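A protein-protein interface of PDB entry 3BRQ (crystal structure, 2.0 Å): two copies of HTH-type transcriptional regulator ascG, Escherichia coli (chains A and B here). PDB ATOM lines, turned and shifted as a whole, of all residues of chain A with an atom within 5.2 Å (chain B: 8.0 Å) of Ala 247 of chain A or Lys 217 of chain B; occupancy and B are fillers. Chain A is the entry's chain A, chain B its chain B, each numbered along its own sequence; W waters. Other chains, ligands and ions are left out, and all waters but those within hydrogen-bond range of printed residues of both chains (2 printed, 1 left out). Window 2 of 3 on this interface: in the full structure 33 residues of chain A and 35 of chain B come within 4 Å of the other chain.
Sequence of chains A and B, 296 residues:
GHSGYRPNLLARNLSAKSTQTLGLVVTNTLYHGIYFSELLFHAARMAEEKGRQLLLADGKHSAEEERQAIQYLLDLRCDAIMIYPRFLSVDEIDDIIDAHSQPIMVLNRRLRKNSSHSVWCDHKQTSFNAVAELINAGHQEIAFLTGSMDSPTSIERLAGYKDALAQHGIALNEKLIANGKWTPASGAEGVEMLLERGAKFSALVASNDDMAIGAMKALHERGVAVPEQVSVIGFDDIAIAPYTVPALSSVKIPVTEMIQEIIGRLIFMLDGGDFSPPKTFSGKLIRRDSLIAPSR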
ATOM      1  N   ALA A 241     -31.274  -3.921   5.877  1.00  0.00           N
ATOM      2  CA  ALA A 241     -31.596  -5.061   6.773  1.00  0.00           C
ATOM      3  C   ALA A 241     -32.241  -6.252   6.028  1.00  0.00           C
ATOM      4  O   ALA A 241     -31.794  -7.372   6.200  1.00  0.00           O
ATOM      5  CB  ALA A 241     -32.487  -4.583   7.892  1.00  0.00           C
ATOM      6  N   PRO A 242     -33.293  -6.024   5.196  1.00  0.00           N
ATOM      7  CA  PRO A 242     -33.873  -7.191   4.539  1.00  0.00           C
ATOM      8  C   PRO A 242     -32.977  -7.858   3.524  1.00  0.00           C
ATOM      9  O   PRO A 242     -33.319  -8.944   3.070  1.00  0.00           O
ATOM     10  CB  PRO A 242     -35.118  -6.632   3.807  1.00  0.00           C
ATOM     11  CG  PRO A 242     -35.380  -5.286   4.352  1.00  0.00           C
ATOM     12  CD  PRO A 242     -34.041  -4.784   4.886  1.00  0.00           C
ATOM     13  N   TYR A 243     -31.847  -7.219   3.181  1.00  0.00           N
ATOM     14  CA  TYR A 243     -30.959  -7.664   2.083  1.00  0.00           C
ATOM     15  C   TYR A 243     -29.646  -8.225   2.616  1.00  0.00           C
ATOM     16  O   TYR A 243     -28.729  -8.568   1.847  1.00  0.00           O
ATOM     17  CB  TYR A 243     -30.755  -6.533   1.058  1.00  0.00           C
ATOM     18  CG  TYR A 243     -32.081  -6.044   0.524  1.00  0.00           C
ATOM     19  CD1 TYR A 243     -32.753  -6.724  -0.478  1.00  0.00           C
ATOM     20  CD2 TYR A 243     -32.683  -4.939   1.077  1.00  0.00           C
ATOM     21  CE1 TYR A 243     -33.996  -6.269  -0.960  1.00  0.00           C
ATOM     22  CE2 TYR A 243     -33.913  -4.506   0.661  1.00  0.00           C
ATOM     23  CZ  TYR A 243     -34.556  -5.167  -0.383  1.00  0.00           C
ATOM     24  OH  TYR A 243     -35.803  -4.721  -0.765  1.00  0.00           O
ATOM     25  N   THR A 244     -29.527  -8.353   3.943  1.00  0.00           N
ATOM     26  CA  THR A 244     -28.344  -9.019   4.454  1.00  0.00           C
ATOM     27  C   THR A 244     -28.503 -10.569   4.328  1.00  0.00           C
ATOM     28  O   THR A 244     -29.592 -11.082   4.039  1.00  0.00           O
ATOM     29  CB  THR A 244     -27.995  -8.575   5.914  1.00  0.00           C
ATOM     30  OG1 THR A 244     -29.102  -8.913   6.752  1.00  0.00           O
ATOM     31  CG2 THR A 244     -27.712  -7.025   5.993  1.00  0.00           C
ATOM     32  N   VAL A 245     -27.405 -11.301   4.520  1.00  0.00           N
ATOM     33  CA  VAL A 245     -27.400 -12.759   4.507  1.00  0.00           C
ATOM     34  C   VAL A 245     -26.924 -13.305   5.882  1.00  0.00           C
ATOM     35  O   VAL A 245     -25.732 -13.246   6.190  1.00  0.00           O
ATOM     36  CB  VAL A 245     -26.472 -13.260   3.383  1.00  0.00           C
ATOM     37  CG1 VAL A 245     -26.363 -14.779   3.391  1.00  0.00           C
ATOM     38  CG2 VAL A 245     -26.980 -12.777   2.041  1.00  0.00           C
ATOM     39  N   PRO A 246     -27.840 -13.807   6.733  1.00  0.00           N
ATOM     40  CA  PRO A 246     -29.285 -13.900   6.599  1.00  0.00           C
ATOM     41  C   PRO A 246     -29.899 -12.501   6.780  1.00  0.00           C
ATOM     42  O   PRO A 246     -29.199 -11.594   7.239  1.00  0.00           O
ATOM     43  CB  PRO A 246     -29.678 -14.847   7.735  1.00  0.00           C
ATOM     44  CG  PRO A 246     -28.635 -14.663   8.783  1.00  0.00           C
ATOM     45  CD  PRO A 246     -27.363 -14.350   8.026  1.00  0.00           C
ATOM     46  N   ALA A 247     -31.152 -12.314   6.381  1.00  0.00           N
ATOM     47  CA  ALA A 247     -31.824 -11.034   6.538  1.00  0.00           C
ATOM     48  C   ALA A 247     -31.966 -10.633   8.029  1.00  0.00           C
ATOM     49  O   ALA A 247     -32.347 -11.449   8.875  1.00  0.00           O
ATOM     50  CB  ALA A 247     -33.152 -11.076   5.864  1.00  0.00           C
ATOM     51  N   LEU A 248     -31.650  -9.374   8.324  1.00  0.00           N
ATOM     52  CA  LEU A 248     -31.426  -8.966   9.693  1.00  0.00           C
ATOM     53  C   LEU A 248     -32.716  -8.582  10.379  1.00  0.00           C
ATOM     54  O   LEU A 248     -33.428  -7.667   9.934  1.00  0.00           O
ATOM     55  CB  LEU A 248     -30.438  -7.773   9.718  1.00  0.00           C
ATOM     56  CG  LEU A 248     -30.308  -7.099  11.096  1.00  0.00           C
ATOM     57  CD1 LEU A 248     -29.769  -8.077  12.165  1.00  0.00           C
ATOM     58  CD2 LEU A 248     -29.389  -5.847  10.927  1.00  0.00           C
ATOM     59  N   SER A 249     -33.012  -9.276  11.474  1.00  0.00           N
ATOM     60  CA  SER A 249     -34.112  -8.914  12.346  1.00  0.00           C
ATOM     61  C   SER A 249     -33.728  -7.644  13.095  1.00  0.00           C
ATOM     62  O   SER A 249     -32.596  -7.505  13.557  1.00  0.00           O
ATOM     63  CB  SER A 249     -34.365 -10.023  13.351  1.00  0.00           C
ATOM     64  OG  SER A 249     -34.605 -11.232  12.651  1.00  0.00           O
ATOM     65  N   ARG A 288     -37.013 -11.406  11.042  1.00  0.00           N
ATOM     66  CA  ARG A 288     -36.527 -11.795   9.732  1.00  0.00           C
ATOM     67  C   ARG A 288     -35.725 -13.096   9.907  1.00  0.00           C
ATOM     68  O   ARG A 288     -35.594 -13.631  11.065  1.00  0.00           O
ATOM     69  CB  ARG A 288     -35.711 -10.642   9.100  1.00  0.00           C
ATOM     70  CG  ARG A 288     -36.573  -9.414   8.761  1.00  0.00           C
ATOM     71  CD  ARG A 288     -35.878  -8.416   7.849  1.00  0.00           C
ATOM     72  NE  ARG A 288     -36.695  -7.204   7.662  1.00  0.00           N
ATOM     73  CZ  ARG A 288     -36.533  -6.043   8.322  1.00  0.00           C
ATOM     74  NH1 ARG A 288     -35.590  -5.894   9.260  1.00  0.00           N
ATOM     75  NH2 ARG A 288     -37.336  -5.014   8.058  1.00  0.00           N
ATOM     76  N   ASP A 289     -35.231 -13.627   8.788  1.00  0.00           N
ATOM     77  CA  ASP A 289     -34.449 -14.891   8.779  1.00  0.00           C
ATOM     78  C   ASP A 289     -33.329 -14.998   9.818  1.00  0.00           C
ATOM     79  O   ASP A 289     -32.872 -16.096  10.099  1.00  0.00           O
ATOM     80  CB  ASP A 289     -33.823 -15.145   7.388  1.00  0.00           C
ATOM     81  CG  ASP A 289     -34.878 -15.387   6.288  1.00  0.00           C
ATOM     82  OD1 ASP A 289     -36.064 -15.706   6.583  1.00  0.00           O
ATOM     83  OD2 ASP A 289     -34.498 -15.247   5.103  1.00  0.00           O
ATOM     84  N   SER A 290     -32.851 -13.884  10.368  1.00  0.00           N
ATOM     85  CA  SER A 290     -31.742 -13.972  11.319  1.00  0.00           C
ATOM     86  C   SER A 290     -32.179 -14.385  12.752  1.00  0.00           C
ATOM     87  O   SER A 290     -31.352 -14.502  13.646  1.00  0.00           O
ATOM     88  CB  SER A 290     -30.997 -12.662  11.405  1.00  0.00           C
ATOM     89  OG  SER A 290     -31.778 -11.708  12.070  1.00  0.00           O
ATOM     90  N   PRO B 184     -31.456  -0.206  -1.686  1.00  0.00           N
ATOM     91  CA  PRO B 184     -31.239  -1.656  -1.712  1.00  0.00           C
ATOM     92  C   PRO B 184     -32.329  -2.384  -2.509  1.00  0.00           C
ATOM     93  O   PRO B 184     -31.970  -3.234  -3.401  1.00  0.00           O
ATOM     94  CB  PRO B 184     -31.293  -2.071  -0.218  1.00  0.00           C
ATOM     95  CG  PRO B 184     -30.903  -0.828   0.550  1.00  0.00           C
ATOM     96  CD  PRO B 184     -31.474   0.332  -0.305  1.00  0.00           C
ATOM     97  N   GLY B 187     -31.808  -2.260  -6.033  1.00  0.00           N
ATOM     98  CA  GLY B 187     -30.711  -3.176  -6.384  1.00  0.00           C
ATOM     99  C   GLY B 187     -31.213  -4.600  -6.607  1.00  0.00           C
ATOM    100  O   GLY B 187     -30.873  -5.268  -7.601  1.00  0.00           O
ATOM    101  N   ALA B 188     -32.015  -5.094  -5.658  1.00  0.00           N
ATOM    102  CA  ALA B 188     -32.521  -6.461  -5.740  1.00  0.00           C
ATOM    103  C   ALA B 188     -33.420  -6.595  -7.002  1.00  0.00           C
ATOM    104  O   ALA B 188     -33.382  -7.606  -7.726  1.00  0.00           O
ATOM    105  CB  ALA B 188     -33.317  -6.805  -4.447  1.00  0.00           C
ATOM    106  N   VAL B 191     -31.520  -6.521 -10.260  1.00  0.00           N
ATOM    107  CA  VAL B 191     -30.935  -7.828 -10.569  1.00  0.00           C
ATOM    108  C   VAL B 191     -31.962  -8.851 -11.029  1.00  0.00           C
ATOM    109  O   VAL B 191     -31.706  -9.577 -11.992  1.00  0.00           O
ATOM    110  CB  VAL B 191     -30.103  -8.427  -9.392  1.00  0.00           C
ATOM    111  CG1 VAL B 191     -30.374  -9.873  -9.268  1.00  0.00           C
ATOM    112  CG2 VAL B 191     -28.612  -8.323  -9.740  1.00  0.00           C
ATOM    113  N   GLU B 192     -33.127  -8.891 -10.367  1.00  0.00           N
ATOM    114  CA  GLU B 192     -34.188  -9.820 -10.771  1.00  0.00           C
ATOM    115  C   GLU B 192     -34.569  -9.488 -12.235  1.00  0.00           C
ATOM    116  O   GLU B 192     -34.781 -10.386 -13.040  1.00  0.00           O
ATOM    117  CB  GLU B 192     -35.384  -9.726  -9.835  1.00  0.00           C
ATOM    118  CG  GLU B 192     -36.469 -10.801 -10.065  1.00  0.00           C
ATOM    119  CD  GLU B 192     -35.876 -12.239 -10.128  1.00  0.00           C
ATOM    120  OE1 GLU B 192     -35.081 -12.620  -9.208  1.00  0.00           O
ATOM    121  OE2 GLU B 192     -36.168 -12.964 -11.117  1.00  0.00           O
ATOM    122  N   ASP B 210     -25.369   0.418  -1.606  1.00  0.00           N
ATOM    123  CA  ASP B 210     -26.752  -0.050  -1.249  1.00  0.00           C
ATOM    124  C   ASP B 210     -27.396  -0.925  -2.297  1.00  0.00           C
ATOM    125  O   ASP B 210     -27.933  -1.961  -1.984  1.00  0.00           O
ATOM    126  CB  ASP B 210     -27.686   1.095  -0.888  1.00  0.00           C
ATOM    127  CG  ASP B 210     -27.388   1.641   0.536  1.00  0.00           C
ATOM    128  OD1 ASP B 210     -26.526   1.078   1.210  1.00  0.00           O
ATOM    129  OD2 ASP B 210     -28.003   2.612   0.985  1.00  0.00           O
ATOM    130  N   MET B 211     -27.362  -0.492  -3.563  1.00  0.00           N
ATOM    131  CA  MET B 211     -27.831  -1.320  -4.618  1.00  0.00           C
ATOM    132  C   MET B 211     -27.003  -2.587  -4.801  1.00  0.00           C
ATOM    133  O   MET B 211     -27.586  -3.627  -5.115  1.00  0.00           O
ATOM    134  CB  MET B 211     -27.894  -0.501  -5.932  1.00  0.00           C
ATOM    135  CG  MET B 211     -28.998   0.635  -5.874  1.00  0.00           C
ATOM    136  SD  MET B 211     -29.124   1.348  -7.720  1.00  0.00           S
ATOM    137  CE  MET B 211     -29.790  -0.124  -8.616  1.00  0.00           C
ATOM    138  N   ALA B 212     -25.677  -2.539  -4.617  1.00  0.00           N
ATOM    139  CA  ALA B 212     -24.831  -3.723  -4.799  1.00  0.00           C
ATOM    140  C   ALA B 212     -25.266  -4.737  -3.715  1.00  0.00           C
ATOM    141  O   ALA B 212     -25.297  -5.921  -3.966  1.00  0.00           O
ATOM    142  CB  ALA B 212     -23.360  -3.384  -4.638  1.00  0.00           C
ATOM    143  N   ILE B 213     -25.594  -4.260  -2.534  1.00  0.00           N
ATOM    144  CA  ILE B 213     -26.010  -5.215  -1.465  1.00  0.00           C
ATOM    145  C   ILE B 213     -27.396  -5.807  -1.790  1.00  0.00           C
ATOM    146  O   ILE B 213     -27.607  -7.027  -1.673  1.00  0.00           O
ATOM    147  CB  ILE B 213     -25.989  -4.569  -0.075  1.00  0.00           C
ATOM    148  CG1 ILE B 213     -24.549  -4.275   0.370  1.00  0.00           C
ATOM    149  CG2 ILE B 213     -26.672  -5.505   1.002  1.00  0.00           C
ATOM    150  CD1 ILE B 213     -24.412  -3.166   1.479  1.00  0.00           C
ATOM    151  N   GLY B 214     -28.309  -4.973  -2.286  1.00  0.00           N
ATOM    152  CA  GLY B 214     -29.588  -5.512  -2.688  1.00  0.00           C
ATOM    153  C   GLY B 214     -29.366  -6.567  -3.730  1.00  0.00           C
ATOM    154  O   GLY B 214     -30.048  -7.615  -3.748  1.00  0.00           O
ATOM    155  N   ALA B 215     -28.451  -6.269  -4.657  1.00  0.00           N
ATOM    156  CA  ALA B 215     -28.216  -7.140  -5.788  1.00  0.00           C
ATOM    157  C   ALA B 215     -27.543  -8.478  -5.372  1.00  0.00           C
ATOM    158  O   ALA B 215     -27.999  -9.535  -5.740  1.00  0.00           O
ATOM    159  CB  ALA B 215     -27.380  -6.353  -6.918  1.00  0.00           C
ATOM    160  N   MET B 216     -26.519  -8.432  -4.518  1.00  0.00           N
ATOM    161  CA  MET B 216     -26.009  -9.656  -3.922  1.00  0.00           C
ATOM    162  C   MET B 216     -27.115 -10.490  -3.227  1.00  0.00           C
ATOM    163  O   MET B 216     -27.049 -11.730  -3.206  1.00  0.00           O
ATOM    164  CB  MET B 216     -24.885  -9.372  -2.931  1.00  0.00           C
ATOM    165  CG  MET B 216     -23.614  -8.984  -3.595  1.00  0.00           C
ATOM    166  SD  MET B 216     -22.074  -8.798  -2.511  1.00  0.00           S
ATOM    167  CE  MET B 216     -22.772  -7.764  -1.026  1.00  0.00           C
ATOM    168  N   LYS B 217     -28.134  -9.841  -2.687  1.00  0.00           N
ATOM    169  CA  LYS B 217     -29.188 -10.602  -1.966  1.00  0.00           C
ATOM    170  C   LYS B 217     -30.035 -11.357  -2.995  1.00  0.00           C
ATOM    171  O   LYS B 217     -30.282 -12.552  -2.904  1.00  0.00           O
ATOM    172  CB  LYS B 217     -30.049  -9.673  -1.067  1.00  0.00           C
ATOM    173  CG  LYS B 217     -31.225 -10.349  -0.369  1.00  0.00           C
ATOM    174  CD  LYS B 217     -30.761 -11.173   0.829  1.00  0.00           C
ATOM    175  CE  LYS B 217     -31.920 -11.811   1.575  1.00  0.00           C
ATOM    176  NZ  LYS B 217     -31.371 -12.680   2.695  1.00  0.00           N
ATOM    177  N   ALA B 218     -30.414 -10.655  -4.035  1.00  0.00           N
ATOM    178  CA  ALA B 218     -31.300 -11.251  -5.034  1.00  0.00           C
ATOM    179  C   ALA B 218     -30.541 -12.372  -5.769  1.00  0.00           C
ATOM    180  O   ALA B 218     -31.131 -13.405  -6.130  1.00  0.00           O
ATOM    181  CB  ALA B 218     -31.825 -10.177  -5.961  1.00  0.00           C
ATOM    182  N   LEU B 219     -29.232 -12.198  -5.920  1.00  0.00           N
ATOM    183  CA  LEU B 219     -28.418 -13.182  -6.589  1.00  0.00           C
ATOM    184  C   LEU B 219     -28.308 -14.458  -5.722  1.00  0.00           C
ATOM    185  O   LEU B 219     -28.487 -15.575  -6.216  1.00  0.00           O
ATOM    186  CB  LEU B 219     -27.020 -12.603  -6.935  1.00  0.00           C
ATOM    187  CG  LEU B 219     -26.880 -11.602  -8.093  1.00  0.00           C
ATOM    188  CD1 LEU B 219     -25.507 -10.947  -8.068  1.00  0.00           C
ATOM    189  CD2 LEU B 219     -27.104 -12.325  -9.428  1.00  0.00           C
ATOM    190  N   HIS B 220     -28.006 -14.273  -4.436  1.00  0.00           N
ATOM    191  CA  HIS B 220     -27.972 -15.361  -3.470  1.00  0.00           C
ATOM    192  C   HIS B 220     -29.300 -16.100  -3.410  1.00  0.00           C
ATOM    193  O   HIS B 220     -29.321 -17.336  -3.338  1.00  0.00           O
ATOM    194  CB  HIS B 220     -27.682 -14.791  -2.097  1.00  0.00           C
ATOM    195  CG  HIS B 220     -27.408 -15.821  -1.056  1.00  0.00           C
ATOM    196  ND1 HIS B 220     -28.323 -16.160  -0.083  1.00  0.00           N
ATOM    197  CD2 HIS B 220     -26.296 -16.548  -0.801  1.00  0.00           C
ATOM    198  CE1 HIS B 220     -27.794 -17.069   0.716  1.00  0.00           C
ATOM    199  NE2 HIS B 220     -26.564 -17.325   0.302  1.00  0.00           N
ATOM    200  N   GLU B 221     -30.404 -15.354  -3.432  1.00  0.00           N
ATOM    201  CA  GLU B 221     -31.745 -15.942  -3.441  1.00  0.00           C
ATOM    202  C   GLU B 221     -32.025 -16.727  -4.724  1.00  0.00           C
ATOM    203  O   GLU B 221     -32.765 -17.698  -4.712  1.00  0.00           O
ATOM    204  CB  GLU B 221     -32.809 -14.870  -3.283  1.00  0.00           C
ATOM    205  CG  GLU B 221     -33.019 -14.355  -1.863  1.00  0.00           C
ATOM    206  CD  GLU B 221     -34.098 -13.276  -1.797  1.00  0.00           C
ATOM    207  OE1 GLU B 221     -34.468 -12.712  -2.871  1.00  0.00           O
ATOM    208  OE2 GLU B 221     -34.579 -12.989  -0.687  1.00  0.00           O
ATOM    209  N   ARG B 222     -31.435 -16.317  -5.842  1.00  0.00           N
ATOM    210  CA  ARG B 222     -31.687 -17.041  -7.064  1.00  0.00           C
ATOM    211  C   ARG B 222     -30.662 -18.165  -7.251  1.00  0.00           C
ATOM    212  O   ARG B 222     -30.615 -18.768  -8.317  1.00  0.00           O
ATOM    213  CB  ARG B 222     -31.754 -16.104  -8.293  1.00  0.00           C
ATOM    214  CG  ARG B 222     -32.921 -15.109  -8.264  1.00  0.00           C
ATOM    215  CD  ARG B 222     -34.254 -15.779  -7.913  1.00  0.00           C
ATOM    216  NE  ARG B 222     -34.799 -16.578  -9.012  1.00  0.00           N
ATOM    217  CZ  ARG B 222     -35.958 -16.332  -9.627  1.00  0.00           C
ATOM    218  NH1 ARG B 222     -36.715 -15.301  -9.246  1.00  0.00           N
ATOM    219  NH2 ARG B 222     -36.370 -17.120 -10.628  1.00  0.00           N
ATOM    220  N   GLY B 223     -29.877 -18.445  -6.202  1.00  0.00           N
ATOM    221  CA  GLY B 223     -28.784 -19.438  -6.258  1.00  0.00           C
ATOM    222  C   GLY B 223     -27.671 -19.089  -7.246  1.00  0.00           C
ATOM    223  O   GLY B 223     -27.067 -19.978  -7.859  1.00  0.00           O
ATOM    224  N   VAL B 224     -27.384 -17.796  -7.396  1.00  0.00           N
ATOM    225  CA  VAL B 224     -26.278 -17.357  -8.278  1.00  0.00           C
ATOM    226  C   VAL B 224     -25.099 -16.962  -7.410  1.00  0.00           C
ATOM    227  O   VAL B 224     -25.173 -15.976  -6.681  1.00  0.00           O
ATOM    228  CB  VAL B 224     -26.672 -16.170  -9.198  1.00  0.00           C
ATOM    229  CG1 VAL B 224     -25.510 -15.789 -10.137  1.00  0.00           C
ATOM    230  CG2 VAL B 224     -27.887 -16.512 -10.037  1.00  0.00           C
ATOM    231  N   VAL B 226     -21.881 -15.463  -5.859  1.00  0.00           N
ATOM    232  CA  VAL B 226     -20.983 -14.312  -5.824  1.00  0.00           C
ATOM    233  C   VAL B 226     -19.768 -14.638  -4.960  1.00  0.00           C
ATOM    234  O   VAL B 226     -19.940 -14.948  -3.767  1.00  0.00           O
ATOM    235  CB  VAL B 226     -21.694 -13.061  -5.251  1.00  0.00           C
ATOM    236  CG1 VAL B 226     -20.760 -11.830  -5.258  1.00  0.00           C
ATOM    237  CG2 VAL B 226     -22.923 -12.760  -6.039  1.00  0.00           C
ATOM    238  N   VAL B 232     -19.292  -8.799  -8.011  1.00  0.00           N
ATOM    239  CA  VAL B 232     -19.995  -7.540  -7.712  1.00  0.00           C
ATOM    240  C   VAL B 232     -19.045  -6.426  -7.179  1.00  0.00           C
ATOM    241  O   VAL B 232     -18.184  -6.657  -6.299  1.00  0.00           O
ATOM    242  CB  VAL B 232     -21.189  -7.811  -6.707  1.00  0.00           C
ATOM    243  CG1 VAL B 232     -22.015  -6.529  -6.379  1.00  0.00           C
ATOM    244  CG2 VAL B 232     -22.093  -8.911  -7.230  1.00  0.00           C
ATOM    245  N   VAL B 245     -21.644 -10.529   3.210  1.00  0.00           N
ATOM    246  CA  VAL B 245     -21.324 -11.927   3.027  1.00  0.00           C
ATOM    247  C   VAL B 245     -21.687 -12.184   1.568  1.00  0.00           C
ATOM    248  O   VAL B 245     -22.879 -12.285   1.261  1.00  0.00           O
ATOM    249  CB  VAL B 245     -22.231 -12.791   3.939  1.00  0.00           C
ATOM    250  CG1 VAL B 245     -22.241 -14.230   3.489  1.00  0.00           C
ATOM    251  CG2 VAL B 245     -21.826 -12.667   5.439  1.00  0.00           C
ATOM    252  N   PRO B 246     -20.702 -12.170   0.644  1.00  0.00           N
ATOM    253  CA  PRO B 246     -19.254 -11.917   0.756  1.00  0.00           C
ATOM    254  C   PRO B 246     -18.962 -10.415   0.879  1.00  0.00           C
ATOM    255  O   PRO B 246     -19.819  -9.568   0.482  1.00  0.00           O
ATOM    256  CB  PRO B 246     -18.704 -12.395  -0.570  1.00  0.00           C
ATOM    257  CG  PRO B 246     -19.888 -12.091  -1.543  1.00  0.00           C
ATOM    258  CD  PRO B 246     -21.137 -12.314  -0.768  1.00  0.00           C
HETATM  259  O   HOH W   1     -26.593  -9.046   0.321  1.00  0.00           O
HETATM  260  O   HOH W   2     -24.751  -9.552   4.020  1.00  0.00           O
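NZ of Lys 217 of chain B lies within hydrogen-bond range of O of Thr 244 of chain A (2.7 Å).
The side-chain hydroxyl (OG1) of Thr 244 of chain A is in hydrogen-bond range of the backbone carbonyl oxygen (O) of Ala 241 of chain A, at 3.2 Å. O of Pro 246 of chain A is in hydrogen-bond range of OG1 of Thr 244 of chain A (2.7 Å). OG1 of Thr 244 of chain A lies within hydrogen-bond range of N of Leu 248 of chain A (3.0 Å). The backbone carbonyl oxygen (O) of Ala 247 of chain A is in hydrogen-bond range of the backbone NH (N) of Ser 290 of chain A, at 2.9 Å.
Among the printed residues, pairs that only touch across the chains: Tyr 243 of chain A with Lys 217 of chain B (3.4 Å), Tyr 243 of chain A with Pro 184 of chain B (3.4 Å), Pro 242 of chain A with Lys 217 of chain B (3.5 Å), Tyr 243 of chain A with Ala 188 of chain B (3.6 Å), Ala 247 of chain A with Lys 217 of chain B (3.7 Å), Tyr 243 of chain A with Ile 213 of chain B (3.8 Å) and Val 245 of chain A with His 220 of chain B (3.8 Å).
Of the printed residues of chain B, Pro 242 of chain A touches Lys 217 (3.5 Å). Of the printed residues of chain B, Thr 244 of chain A touches Lys 217. Of the printed residues of chain B, Val 245 of chain A touches His 220 (3.8 Å). Ala 247 of chain A touches just one residue of chain B: Lys 217. Glu 192 of chain B touches none of the printed residues of chain A. Lys 217 of chain B touches just these residues of chain A: Pro 242, Tyr 243, Thr 244 and Ala 247. Val 224 of chain B touches none of the printed residues of chain A. The nearest residue of chain A that does not touch Lys 217 of chain B is Val 245 of chain A (4.3 Å). The nearest printed residue of chain A that does not touch Pro 184 of chain B is Ala 241 of chain A (6.2 Å).
Printed residues of chain B that touch a printed residue of chain A: Pro 184, Ala 188, Ile 213, Lys 217 and His 220. Among the printed residues, no Asp or Glu carboxylate lies within 4 Å of a Lys or Arg side-chain nitrogen of the other chain.
2 positions are printed for both chains.
Water W1 lies within hydrogen-bond range of O of Tyr 243 of chain A (2.7 Å), O of Ile 213 of chain B (3.0 Å) and N of Lys 217 of chain B (3.5 Å). Water W2 bridges the backbone NH of Val 245 of chain A (3.2 Å) and the backbone NH of Val 245 of chain B (3.4 Å).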
